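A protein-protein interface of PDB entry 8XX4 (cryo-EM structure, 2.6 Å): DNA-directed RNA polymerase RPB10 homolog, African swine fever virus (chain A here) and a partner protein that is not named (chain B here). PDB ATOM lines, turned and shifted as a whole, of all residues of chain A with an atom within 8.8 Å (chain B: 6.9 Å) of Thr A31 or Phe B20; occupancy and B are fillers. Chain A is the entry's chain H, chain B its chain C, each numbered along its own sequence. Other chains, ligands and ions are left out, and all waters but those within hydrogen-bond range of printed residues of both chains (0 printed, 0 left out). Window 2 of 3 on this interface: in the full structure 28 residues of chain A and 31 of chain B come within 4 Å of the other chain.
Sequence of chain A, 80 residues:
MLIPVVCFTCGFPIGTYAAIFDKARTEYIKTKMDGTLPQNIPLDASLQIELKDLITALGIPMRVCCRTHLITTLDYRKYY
O of Tyr A28 sits at hydrogen-bond distance from OG1 of Thr A31 (3.5 Å).
Among the printed residues, pairs that only touch across the chains: Ile A20 with Ile B21, Ile A20 with Ala B24, Ala A24 with Phe B20, Ala A24 with Ile B21, Ala A24 with Ala B24, Tyr A28 with Phe B20, Thr A31 with Phe B20, Leu A54 with Asn B18, Leu A54 with Phe B20, Leu A54 with Ile B21, Ala A57 with Asn B18 and Leu A58 with Ile B21.
Of the printed residues of chain B, Ile A20 touches Ile B21 and Ala B24.
Printed residues of chain B within 4 Å of Ala A24: Phe B20, Ile B21 and Ala B24.
Of the printed residues of chain B, Tyr A28 touches Phe B20.
Printed residues of chain B within 4 Å of Leu A54: Asn B18 (3.5 Å), Phe B20 (3.97 Å) and Ile B21 (3.9 Å).
Printed residues of chain B within 4 Å of Ala A57: Asn B18 (3.6 Å).
Phe B20 touches just these residues of chain A: Ala A24 (3.6 Å), Tyr A28 (3.4 Å), Thr A31 (3.8 Å) and Leu A54 (3.97 Å).
The nearest printed residue of chain B that does not touch Leu A58 is Asn B18 (6.3 Å).
Of the 20 printed residues of chain A, 7 touch a printed residue of chain B.
Printed residues of chain A that touch a printed residue of chain B: Ile A20, Ala A24, Tyr A28, Thr A31, Leu A54, Ala A57 and Leu A58.
Hydrophobic or aromatic side chains of chain A that line the printed part of chain B: Ile A20, Ala A24, Tyr A28, Leu A54, Ala A57 and Leu A58.
Hydrophobic or aromatic side chains of chain B within 4 Å of the printed part of chain A: Phe B20, Ile B21 and Ala B24.
Along chain B the printed residues that touch a printed residue of chain A span positions 18 to 24.
Among the printed residues, 12 pairs touch across the chains.
Among the printed residues, no Asp or Glu carboxylate lies within 4 Å of a Lys or Arg side-chain nitrogen of the other chain.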
ATOM      1  N   ALA A  19      -6.690  -5.247  18.312  1.00  0.00           N
ATOM      2  CA  ALA A  19      -7.825  -6.011  17.794  1.00  0.00           C
ATOM      3  C   ALA A  19      -9.151  -5.347  18.138  1.00  0.00           C
ATOM      4  O   ALA A  19     -10.044  -5.232  17.281  1.00  0.00           O
ATOM      5  CB  ALA A  19      -7.787  -7.433  18.345  1.00  0.00           C
ATOM      6  N   ILE A  20      -9.302  -4.925  19.394  1.00  0.00           N
ATOM      7  CA  ILE A  20     -10.508  -4.223  19.809  1.00  0.00           C
ATOM      8  C   ILE A  20     -10.698  -2.977  18.966  1.00  0.00           C
ATOM      9  O   ILE A  20     -11.812  -2.670  18.535  1.00  0.00           O
ATOM     10  CB  ILE A  20     -10.445  -3.888  21.310  1.00  0.00           C
ATOM     11  CG1 ILE A  20     -10.352  -5.166  22.140  1.00  0.00           C
ATOM     12  CG2 ILE A  20     -11.652  -3.077  21.727  1.00  0.00           C
ATOM     13  CD1 ILE A  20      -9.810  -4.951  23.532  1.00  0.00           C
ATOM     14  N   PHE A  21      -9.612  -2.246  18.703  1.00  0.00           N
ATOM     15  CA  PHE A  21      -9.709  -1.052  17.880  1.00  0.00           C
ATOM     16  C   PHE A  21     -10.149  -1.391  16.470  1.00  0.00           C
ATOM     17  O   PHE A  21     -11.000  -0.705  15.905  1.00  0.00           O
ATOM     18  CB  PHE A  21      -8.375  -0.318  17.832  1.00  0.00           C
ATOM     19  CG  PHE A  21      -8.350   0.786  16.827  1.00  0.00           C
ATOM     20  CD1 PHE A  21      -9.072   1.943  17.041  1.00  0.00           C
ATOM     21  CD2 PHE A  21      -7.633   0.658  15.656  1.00  0.00           C
ATOM     22  CE1 PHE A  21      -9.064   2.950  16.118  1.00  0.00           C
ATOM     23  CE2 PHE A  21      -7.626   1.663  14.731  1.00  0.00           C
ATOM     24  CZ  PHE A  21      -8.340   2.810  14.962  1.00  0.00           C
ATOM     25  N   ASP A  22      -9.573  -2.437  15.877  1.00  0.00           N
ATOM     26  CA  ASP A  22      -9.935  -2.793  14.510  1.00  0.00           C
ATOM     27  C   ASP A  22     -11.423  -3.084  14.396  1.00  0.00           C
ATOM     28  O   ASP A  22     -12.121  -2.521  13.540  1.00  0.00           O
ATOM     29  CB  ASP A  22      -9.121  -3.999  14.051  1.00  0.00           C
ATOM     30  CG  ASP A  22      -9.099  -4.147  12.546  1.00  0.00           C
ATOM     31  OD1 ASP A  22      -9.773  -3.352  11.858  1.00  0.00           O
ATOM     32  OD2 ASP A  22      -8.415  -5.064  12.048  1.00  0.00           O
ATOM     33  N   LYS A  23     -11.936  -3.953  15.264  1.00  0.00           N
ATOM     34  CA  LYS A  23     -13.337  -4.342  15.129  1.00  0.00           C
ATOM     35  C   LYS A  23     -14.280  -3.223  15.553  1.00  0.00           C
ATOM     36  O   LYS A  23     -15.320  -3.007  14.915  1.00  0.00           O
ATOM     37  CB  LYS A  23     -13.596  -5.620  15.906  1.00  0.00           C
ATOM     38  CG  LYS A  23     -12.435  -6.577  15.831  1.00  0.00           C
ATOM     39  CD  LYS A  23     -12.436  -7.390  14.552  1.00  0.00           C
ATOM     40  CE  LYS A  23     -11.264  -8.360  14.534  1.00  0.00           C
ATOM     41  NZ  LYS A  23      -9.982  -7.673  14.211  1.00  0.00           N
ATOM     42  N   ALA A  24     -13.936  -2.484  16.609  1.00  0.00           N
ATOM     43  CA  ALA A  24     -14.757  -1.351  17.007  1.00  0.00           C
ATOM     44  C   ALA A  24     -14.755  -0.271  15.939  1.00  0.00           C
ATOM     45  O   ALA A  24     -15.755   0.421  15.750  1.00  0.00           O
ATOM     46  CB  ALA A  24     -14.264  -0.791  18.338  1.00  0.00           C
ATOM     47  N   ARG A  25     -13.644  -0.118  15.218  1.00  0.00           N
ATOM     48  CA  ARG A  25     -13.577   0.869  14.150  1.00  0.00           C
ATOM     49  C   ARG A  25     -14.422   0.447  12.964  1.00  0.00           C
ATOM     50  O   ARG A  25     -15.103   1.278  12.358  1.00  0.00           O
ATOM     51  CB  ARG A  25     -12.128   1.087  13.723  1.00  0.00           C
ATOM     52  CG  ARG A  25     -11.970   2.027  12.550  1.00  0.00           C
ATOM     53  CD  ARG A  25     -10.538   2.067  12.069  1.00  0.00           C
ATOM     54  NE  ARG A  25      -9.979   0.732  11.913  1.00  0.00           N
ATOM     55  CZ  ARG A  25      -8.723   0.484  11.571  1.00  0.00           C
ATOM     56  NH1 ARG A  25      -7.864   1.462  11.339  1.00  0.00           N
ATOM     57  NH2 ARG A  25      -8.318  -0.778  11.457  1.00  0.00           N
ATOM     58  N   THR A  26     -14.396  -0.839  12.614  1.00  0.00           N
ATOM     59  CA  THR A  26     -15.288  -1.314  11.561  1.00  0.00           C
ATOM     60  C   THR A  26     -16.745  -1.073  11.940  1.00  0.00           C
ATOM     61  O   THR A  26     -17.536  -0.560  11.137  1.00  0.00           O
ATOM     62  CB  THR A  26     -15.036  -2.795  11.285  1.00  0.00           C
ATOM     63  OG1 THR A  26     -13.746  -2.956  10.684  1.00  0.00           O
ATOM     64  CG2 THR A  26     -16.091  -3.344  10.346  1.00  0.00           C
ATOM     65  N   GLU A  27     -17.105  -1.397  13.186  1.00  0.00           N
ATOM     66  CA  GLU A  27     -18.470  -1.165  13.648  1.00  0.00           C
ATOM     67  C   GLU A  27     -18.827   0.316  13.612  1.00  0.00           C
ATOM     68  O   GLU A  27     -19.899   0.692  13.132  1.00  0.00           O
ATOM     69  CB  GLU A  27     -18.642  -1.710  15.066  1.00  0.00           C
ATOM     70  CG  GLU A  27     -18.856  -3.215  15.173  1.00  0.00           C
ATOM     71  CD  GLU A  27     -19.327  -3.856  13.883  1.00  0.00           C
ATOM     72  OE1 GLU A  27     -18.580  -4.683  13.319  1.00  0.00           O
ATOM     73  OE2 GLU A  27     -20.460  -3.559  13.449  1.00  0.00           O
ATOM     74  N   TYR A  28     -17.931   1.173  14.102  1.00  0.00           N
ATOM     75  CA  TYR A  28     -18.233   2.591  14.233  1.00  0.00           C
ATOM     76  C   TYR A  28     -18.290   3.270  12.876  1.00  0.00           C
ATOM     77  O   TYR A  28     -19.037   4.237  12.699  1.00  0.00           O
ATOM     78  CB  TYR A  28     -17.194   3.247  15.146  1.00  0.00           C
ATOM     79  CG  TYR A  28     -17.252   4.754  15.234  1.00  0.00           C
ATOM     80  CD1 TYR A  28     -16.615   5.556  14.304  1.00  0.00           C
ATOM     81  CD2 TYR A  28     -17.951   5.374  16.257  1.00  0.00           C
ATOM     82  CE1 TYR A  28     -16.671   6.926  14.397  1.00  0.00           C
ATOM     83  CE2 TYR A  28     -18.014   6.742  16.352  1.00  0.00           C
ATOM     84  CZ  TYR A  28     -17.374   7.514  15.419  1.00  0.00           C
ATOM     85  OH  TYR A  28     -17.432   8.883  15.508  1.00  0.00           O
ATOM     86  N   ILE A  29     -17.508   2.786  11.913  1.00  0.00           N
ATOM     87  CA  ILE A  29     -17.609   3.289  10.552  1.00  0.00           C
ATOM     88  C   ILE A  29     -18.922   2.846   9.925  1.00  0.00           C
ATOM     89  O   ILE A  29     -19.577   3.616   9.215  1.00  0.00           O
ATOM     90  CB  ILE A  29     -16.393   2.832   9.729  1.00  0.00           C
ATOM     91  CG1 ILE A  29     -15.148   3.602  10.160  1.00  0.00           C
ATOM     92  CG2 ILE A  29     -16.635   3.029   8.248  1.00  0.00           C
ATOM     93  CD1 ILE A  29     -13.873   3.043   9.594  1.00  0.00           C
ATOM     94  N   LYS A  30     -19.343   1.607  10.198  1.00  0.00           N
ATOM     95  CA  LYS A  30     -20.584   1.110   9.609  1.00  0.00           C
ATOM     96  C   LYS A  30     -21.785   1.946  10.035  1.00  0.00           C
ATOM     97  O   LYS A  30     -22.655   2.253   9.211  1.00  0.00           O
ATOM     98  CB  LYS A  30     -20.786  -0.357   9.977  1.00  0.00           C
ATOM     99  CG  LYS A  30     -20.987  -1.260   8.775  1.00  0.00           C
ATOM    100  CD  LYS A  30     -20.403  -2.640   9.012  1.00  0.00           C
ATOM    101  CE  LYS A  30     -20.864  -3.218  10.337  1.00  0.00           C
ATOM    102  NZ  LYS A  30     -20.385  -4.615  10.522  1.00  0.00           N
ATOM    103  N   THR A  31     -21.859   2.326  11.311  1.00  0.00           N
ATOM    104  CA  THR A  31     -22.987   3.139  11.756  1.00  0.00           C
ATOM    105  C   THR A  31     -22.864   4.585  11.297  1.00  0.00           C
ATOM    106  O   THR A  31     -23.875   5.284  11.186  1.00  0.00           O
ATOM    107  CB  THR A  31     -23.128   3.089  13.278  1.00  0.00           C
ATOM    108  OG1 THR A  31     -22.283   4.078  13.876  1.00  0.00           O
ATOM    109  CG2 THR A  31     -22.765   1.716  13.809  1.00  0.00           C
ATOM    110  N   LYS A  32     -21.647   5.055  11.031  1.00  0.00           N
ATOM    111  CA  LYS A  32     -21.458   6.438  10.611  1.00  0.00           C
ATOM    112  C   LYS A  32     -21.827   6.672   9.155  1.00  0.00           C
ATOM    113  O   LYS A  32     -21.993   7.827   8.754  1.00  0.00           O
ATOM    114  CB  LYS A  32     -20.010   6.866  10.849  1.00  0.00           C
ATOM    115  CG  LYS A  32     -19.747   7.367  12.251  1.00  0.00           C
ATOM    116  CD  LYS A  32     -20.197   8.800  12.416  1.00  0.00           C
ATOM    117  CE  LYS A  32     -20.348   9.156  13.880  1.00  0.00           C
ATOM    118  NZ  LYS A  32     -20.893   8.016  14.665  1.00  0.00           N
ATOM    119  N   MET A  33     -21.951   5.619   8.355  1.00  0.00           N
ATOM    120  CA  MET A  33     -22.393   5.767   6.973  1.00  0.00           C
ATOM    121  C   MET A  33     -23.904   5.601   6.872  1.00  0.00           C
ATOM    122  O   MET A  33     -24.395   4.662   6.248  1.00  0.00           O
ATOM    123  CB  MET A  33     -21.695   4.757   6.058  1.00  0.00           C
ATOM    124  CG  MET A  33     -20.225   4.530   6.365  1.00  0.00           C
ATOM    125  SD  MET A  33     -19.304   6.050   6.664  1.00  0.00           S
ATOM    126  CE  MET A  33     -18.748   6.442   5.008  1.00  0.00           C
ATOM    127  N   ILE A  49     -13.539   9.641   8.931  1.00  0.00           N
ATOM    128  CA  ILE A  49     -14.303   9.583  10.169  1.00  0.00           C
ATOM    129  C   ILE A  49     -13.349   9.699  11.349  1.00  0.00           C
ATOM    130  O   ILE A  49     -12.345   8.979  11.429  1.00  0.00           O
ATOM    131  CB  ILE A  49     -15.120   8.284  10.237  1.00  0.00           C
ATOM    132  CG1 ILE A  49     -15.905   8.071   8.940  1.00  0.00           C
ATOM    133  CG2 ILE A  49     -16.058   8.325  11.415  1.00  0.00           C
ATOM    134  CD1 ILE A  49     -17.280   8.699   8.932  1.00  0.00           C
ATOM    135  N   ASP A  53     -12.432   9.821  19.734  1.00  0.00           N
ATOM    136  CA  ASP A  53     -13.201   9.317  20.865  1.00  0.00           C
ATOM    137  C   ASP A  53     -13.021   7.815  21.039  1.00  0.00           C
ATOM    138  O   ASP A  53     -12.900   7.329  22.168  1.00  0.00           O
ATOM    139  CB  ASP A  53     -14.676   9.662  20.683  1.00  0.00           C
ATOM    140  CG  ASP A  53     -14.928  11.154  20.688  1.00  0.00           C
ATOM    141  OD1 ASP A  53     -14.103  11.896  21.260  1.00  0.00           O
ATOM    142  OD2 ASP A  53     -15.950  11.582  20.117  1.00  0.00           O
ATOM    143  N   LEU A  54     -13.007   7.066  19.937  1.00  0.00           N
ATOM    144  CA  LEU A  54     -12.841   5.619  20.014  1.00  0.00           C
ATOM    145  C   LEU A  54     -11.503   5.250  20.643  1.00  0.00           C
ATOM    146  O   LEU A  54     -11.431   4.406  21.545  1.00  0.00           O
ATOM    147  CB  LEU A  54     -12.958   5.020  18.614  1.00  0.00           C
ATOM    148  CG  LEU A  54     -13.763   3.738  18.440  1.00  0.00           C
ATOM    149  CD1 LEU A  54     -15.238   4.027  18.618  1.00  0.00           C
ATOM    150  CD2 LEU A  54     -13.499   3.159  17.070  1.00  0.00           C
ATOM    151  N   ALA A  57     -11.405   6.181  24.342  1.00  0.00           N
ATOM    152  CA  ALA A  57     -12.132   5.186  25.118  1.00  0.00           C
ATOM    153  C   ALA A  57     -11.355   3.886  25.220  1.00  0.00           C
ATOM    154  O   ALA A  57     -11.539   3.129  26.176  1.00  0.00           O
ATOM    155  CB  ALA A  57     -13.503   4.933  24.499  1.00  0.00           C
ATOM    156  N   LEU A  58     -10.493   3.608  24.246  1.00  0.00           N
ATOM    157  CA  LEU A  58      -9.643   2.428  24.337  1.00  0.00           C
ATOM    158  C   LEU A  58      -8.623   2.542  25.461  1.00  0.00           C
ATOM    159  O   LEU A  58      -8.100   1.525  25.924  1.00  0.00           O
ATOM    160  CB  LEU A  58      -8.927   2.208  23.014  1.00  0.00           C
ATOM    161  CG  LEU A  58      -9.537   1.150  22.118  1.00  0.00           C
ATOM    162  CD1 LEU A  58      -8.613   0.963  20.962  1.00  0.00           C
ATOM    163  CD2 LEU A  58      -9.740  -0.142  22.875  1.00  0.00           C
ATOM    164  N   PHE B  16     -15.430   1.345  29.013  1.00  0.00           N
ATOM    165  CA  PHE B  16     -16.448   0.438  28.510  1.00  0.00           C
ATOM    166  C   PHE B  16     -17.806   1.106  28.337  1.00  0.00           C
ATOM    167  O   PHE B  16     -18.736   0.461  27.845  1.00  0.00           O
ATOM    168  CB  PHE B  16     -16.568  -0.773  29.432  1.00  0.00           C
ATOM    169  CG  PHE B  16     -15.456  -1.762  29.262  1.00  0.00           C
ATOM    170  CD1 PHE B  16     -15.397  -2.568  28.143  1.00  0.00           C
ATOM    171  CD2 PHE B  16     -14.460  -1.874  30.213  1.00  0.00           C
ATOM    172  CE1 PHE B  16     -14.373  -3.471  27.981  1.00  0.00           C
ATOM    173  CE2 PHE B  16     -13.434  -2.777  30.054  1.00  0.00           C
ATOM    174  CZ  PHE B  16     -13.390  -3.576  28.937  1.00  0.00           C
ATOM    175  N   SER B  17     -17.944   2.373  28.730  1.00  0.00           N
ATOM    176  CA  SER B  17     -19.153   3.117  28.408  1.00  0.00           C
ATOM    177  C   SER B  17     -19.258   3.411  26.920  1.00  0.00           C
ATOM    178  O   SER B  17     -20.331   3.805  26.454  1.00  0.00           O
ATOM    179  CB  SER B  17     -19.201   4.425  29.196  1.00  0.00           C
ATOM    180  OG  SER B  17     -18.570   5.470  28.479  1.00  0.00           O
ATOM    181  N   ASN B  18     -18.170   3.248  26.174  1.00  0.00           N
ATOM    182  CA  ASN B  18     -18.222   3.357  24.722  1.00  0.00           C
ATOM    183  C   ASN B  18     -18.809   2.076  24.151  1.00  0.00           C
ATOM    184  O   ASN B  18     -18.267   0.988  24.367  1.00  0.00           O
ATOM    185  CB  ASN B  18     -16.828   3.611  24.160  1.00  0.00           C
ATOM    186  CG  ASN B  18     -16.858   4.200  22.767  1.00  0.00           C
ATOM    187  OD1 ASN B  18     -16.706   3.488  21.778  1.00  0.00           O
ATOM    188  ND2 ASN B  18     -17.046   5.509  22.681  1.00  0.00           N
ATOM    189  N   LEU B  19     -19.920   2.205  23.424  1.00  0.00           N
ATOM    190  CA  LEU B  19     -20.648   1.023  22.979  1.00  0.00           C
ATOM    191  C   LEU B  19     -19.810   0.169  22.038  1.00  0.00           C
ATOM    192  O   LEU B  19     -19.802  -1.061  22.151  1.00  0.00           O
ATOM    193  CB  LEU B  19     -21.958   1.437  22.311  1.00  0.00           C
ATOM    194  CG  LEU B  19     -23.218   1.359  23.177  1.00  0.00           C
ATOM    195  CD1 LEU B  19     -22.958   1.879  24.582  1.00  0.00           C
ATOM    196  CD2 LEU B  19     -24.355   2.127  22.533  1.00  0.00           C
ATOM    197  N   PHE B  20     -19.100   0.800  21.103  1.00  0.00           N
ATOM    198  CA  PHE B  20     -18.311   0.041  20.136  1.00  0.00           C
ATOM    199  C   PHE B  20     -17.160  -0.693  20.810  1.00  0.00           C
ATOM    200  O   PHE B  20     -16.906  -1.867  20.514  1.00  0.00           O
ATOM    201  CB  PHE B  20     -17.795   0.975  19.046  1.00  0.00           C
ATOM    202  CG  PHE B  20     -18.851   1.867  18.470  1.00  0.00           C
ATOM    203  CD1 PHE B  20     -19.621   1.448  17.403  1.00  0.00           C
ATOM    204  CD2 PHE B  20     -19.084   3.120  19.006  1.00  0.00           C
ATOM    205  CE1 PHE B  20     -20.595   2.264  16.876  1.00  0.00           C
ATOM    206  CE2 PHE B  20     -20.056   3.937  18.484  1.00  0.00           C
ATOM    207  CZ  PHE B  20     -20.812   3.510  17.415  1.00  0.00           C
ATOM    208  N   ILE B  21     -16.459  -0.019  21.723  1.00  0.00           N
ATOM    209  CA  ILE B  21     -15.351  -0.650  22.434  1.00  0.00           C
ATOM    210  C   ILE B  21     -15.851  -1.850  23.226  1.00  0.00           C
ATOM    211  O   ILE B  21     -15.273  -2.943  23.170  1.00  0.00           O
ATOM    212  CB  ILE B  21     -14.653   0.370  23.351  1.00  0.00           C
ATOM    213  CG1 ILE B  21     -13.910   1.430  22.537  1.00  0.00           C
ATOM    214  CG2 ILE B  21     -13.714  -0.333  24.303  1.00  0.00           C
ATOM    215  CD1 ILE B  21     -13.152   0.887  21.365  1.00  0.00           C
ATOM    216  N   LYS B  22     -16.937  -1.658  23.978  1.00  0.00           N
ATOM    217  CA  LYS B  22     -17.475  -2.734  24.799  1.00  0.00           C
ATOM    218  C   LYS B  22     -17.946  -3.897  23.940  1.00  0.00           C
ATOM    219  O   LYS B  22     -17.694  -5.062  24.268  1.00  0.00           O
ATOM    220  CB  LYS B  22     -18.613  -2.204  25.669  1.00  0.00           C
ATOM    221  CG  LYS B  22     -19.238  -3.246  26.573  1.00  0.00           C
ATOM    222  CD  LYS B  22     -20.366  -2.657  27.402  1.00  0.00           C
ATOM    223  CE  LYS B  22     -19.968  -2.552  28.865  1.00  0.00           C
ATOM    224  NZ  LYS B  22     -20.382  -1.260  29.475  1.00  0.00           N
ATOM    225  N   ASN B  23     -18.619  -3.600  22.829  1.00  0.00           N
ATOM    226  CA  ASN B  23     -19.112  -4.654  21.953  1.00  0.00           C
ATOM    227  C   ASN B  23     -17.964  -5.467  21.369  1.00  0.00           C
ATOM    228  O   ASN B  23     -18.013  -6.702  21.347  1.00  0.00           O
ATOM    229  CB  ASN B  23     -19.961  -4.046  20.839  1.00  0.00           C
ATOM    230  CG  ASN B  23     -21.325  -3.625  21.321  1.00  0.00           C
ATOM    231  OD1 ASN B  23     -21.872  -4.210  22.253  1.00  0.00           O
ATOM    232  ND2 ASN B  23     -21.884  -2.598  20.692  1.00  0.00           N
ATOM    233  N   ALA B  24     -16.914  -4.789  20.897  1.00  0.00           N
ATOM    234  CA  ALA B  24     -15.783  -5.506  20.317  1.00  0.00           C
ATOM    235  C   ALA B  24     -15.068  -6.355  21.362  1.00  0.00           C
ATOM    236  O   ALA B  24     -14.754  -7.529  21.112  1.00  0.00           O
ATOM    237  CB  ALA B  24     -14.816  -4.520  19.669  1.00  0.00           C
ATOM    238  N   ALA B  25     -14.811  -5.785  22.542  1.00  0.00           N
ATOM    239  CA  ALA B  25     -14.130  -6.540  23.587  1.00  0.00           C
ATOM    240  C   ALA B  25     -14.948  -7.757  23.993  1.00  0.00           C
ATOM    241  O   ALA B  25     -14.411  -8.859  24.134  1.00  0.00           O
ATOM    242  CB  ALA B  25     -13.855  -5.642  24.791  1.00  0.00           C
ATOM    243  N   LYS B  26     -16.261  -7.582  24.155  1.00  0.00           N
ATOM    244  CA  LYS B  26     -17.116  -8.705  24.510  1.00  0.00           C
ATOM    245  C   LYS B  26     -17.111  -9.775  23.428  1.00  0.00           C
ATOM    246  O   LYS B  26     -16.997 -10.967  23.730  1.00  0.00           O
ATOM    247  CB  LYS B  26     -18.539  -8.213  24.762  1.00  0.00           C
ATOM    248  CG  LYS B  26     -19.403  -9.184  25.539  1.00  0.00           C
ATOM    249  CD  LYS B  26     -18.732  -9.615  26.827  1.00  0.00           C
ATOM    250  CE  LYS B  26     -19.578 -10.631  27.569  1.00  0.00           C
ATOM    251  NZ  LYS B  26     -20.508 -11.344  26.652  1.00  0.00           N
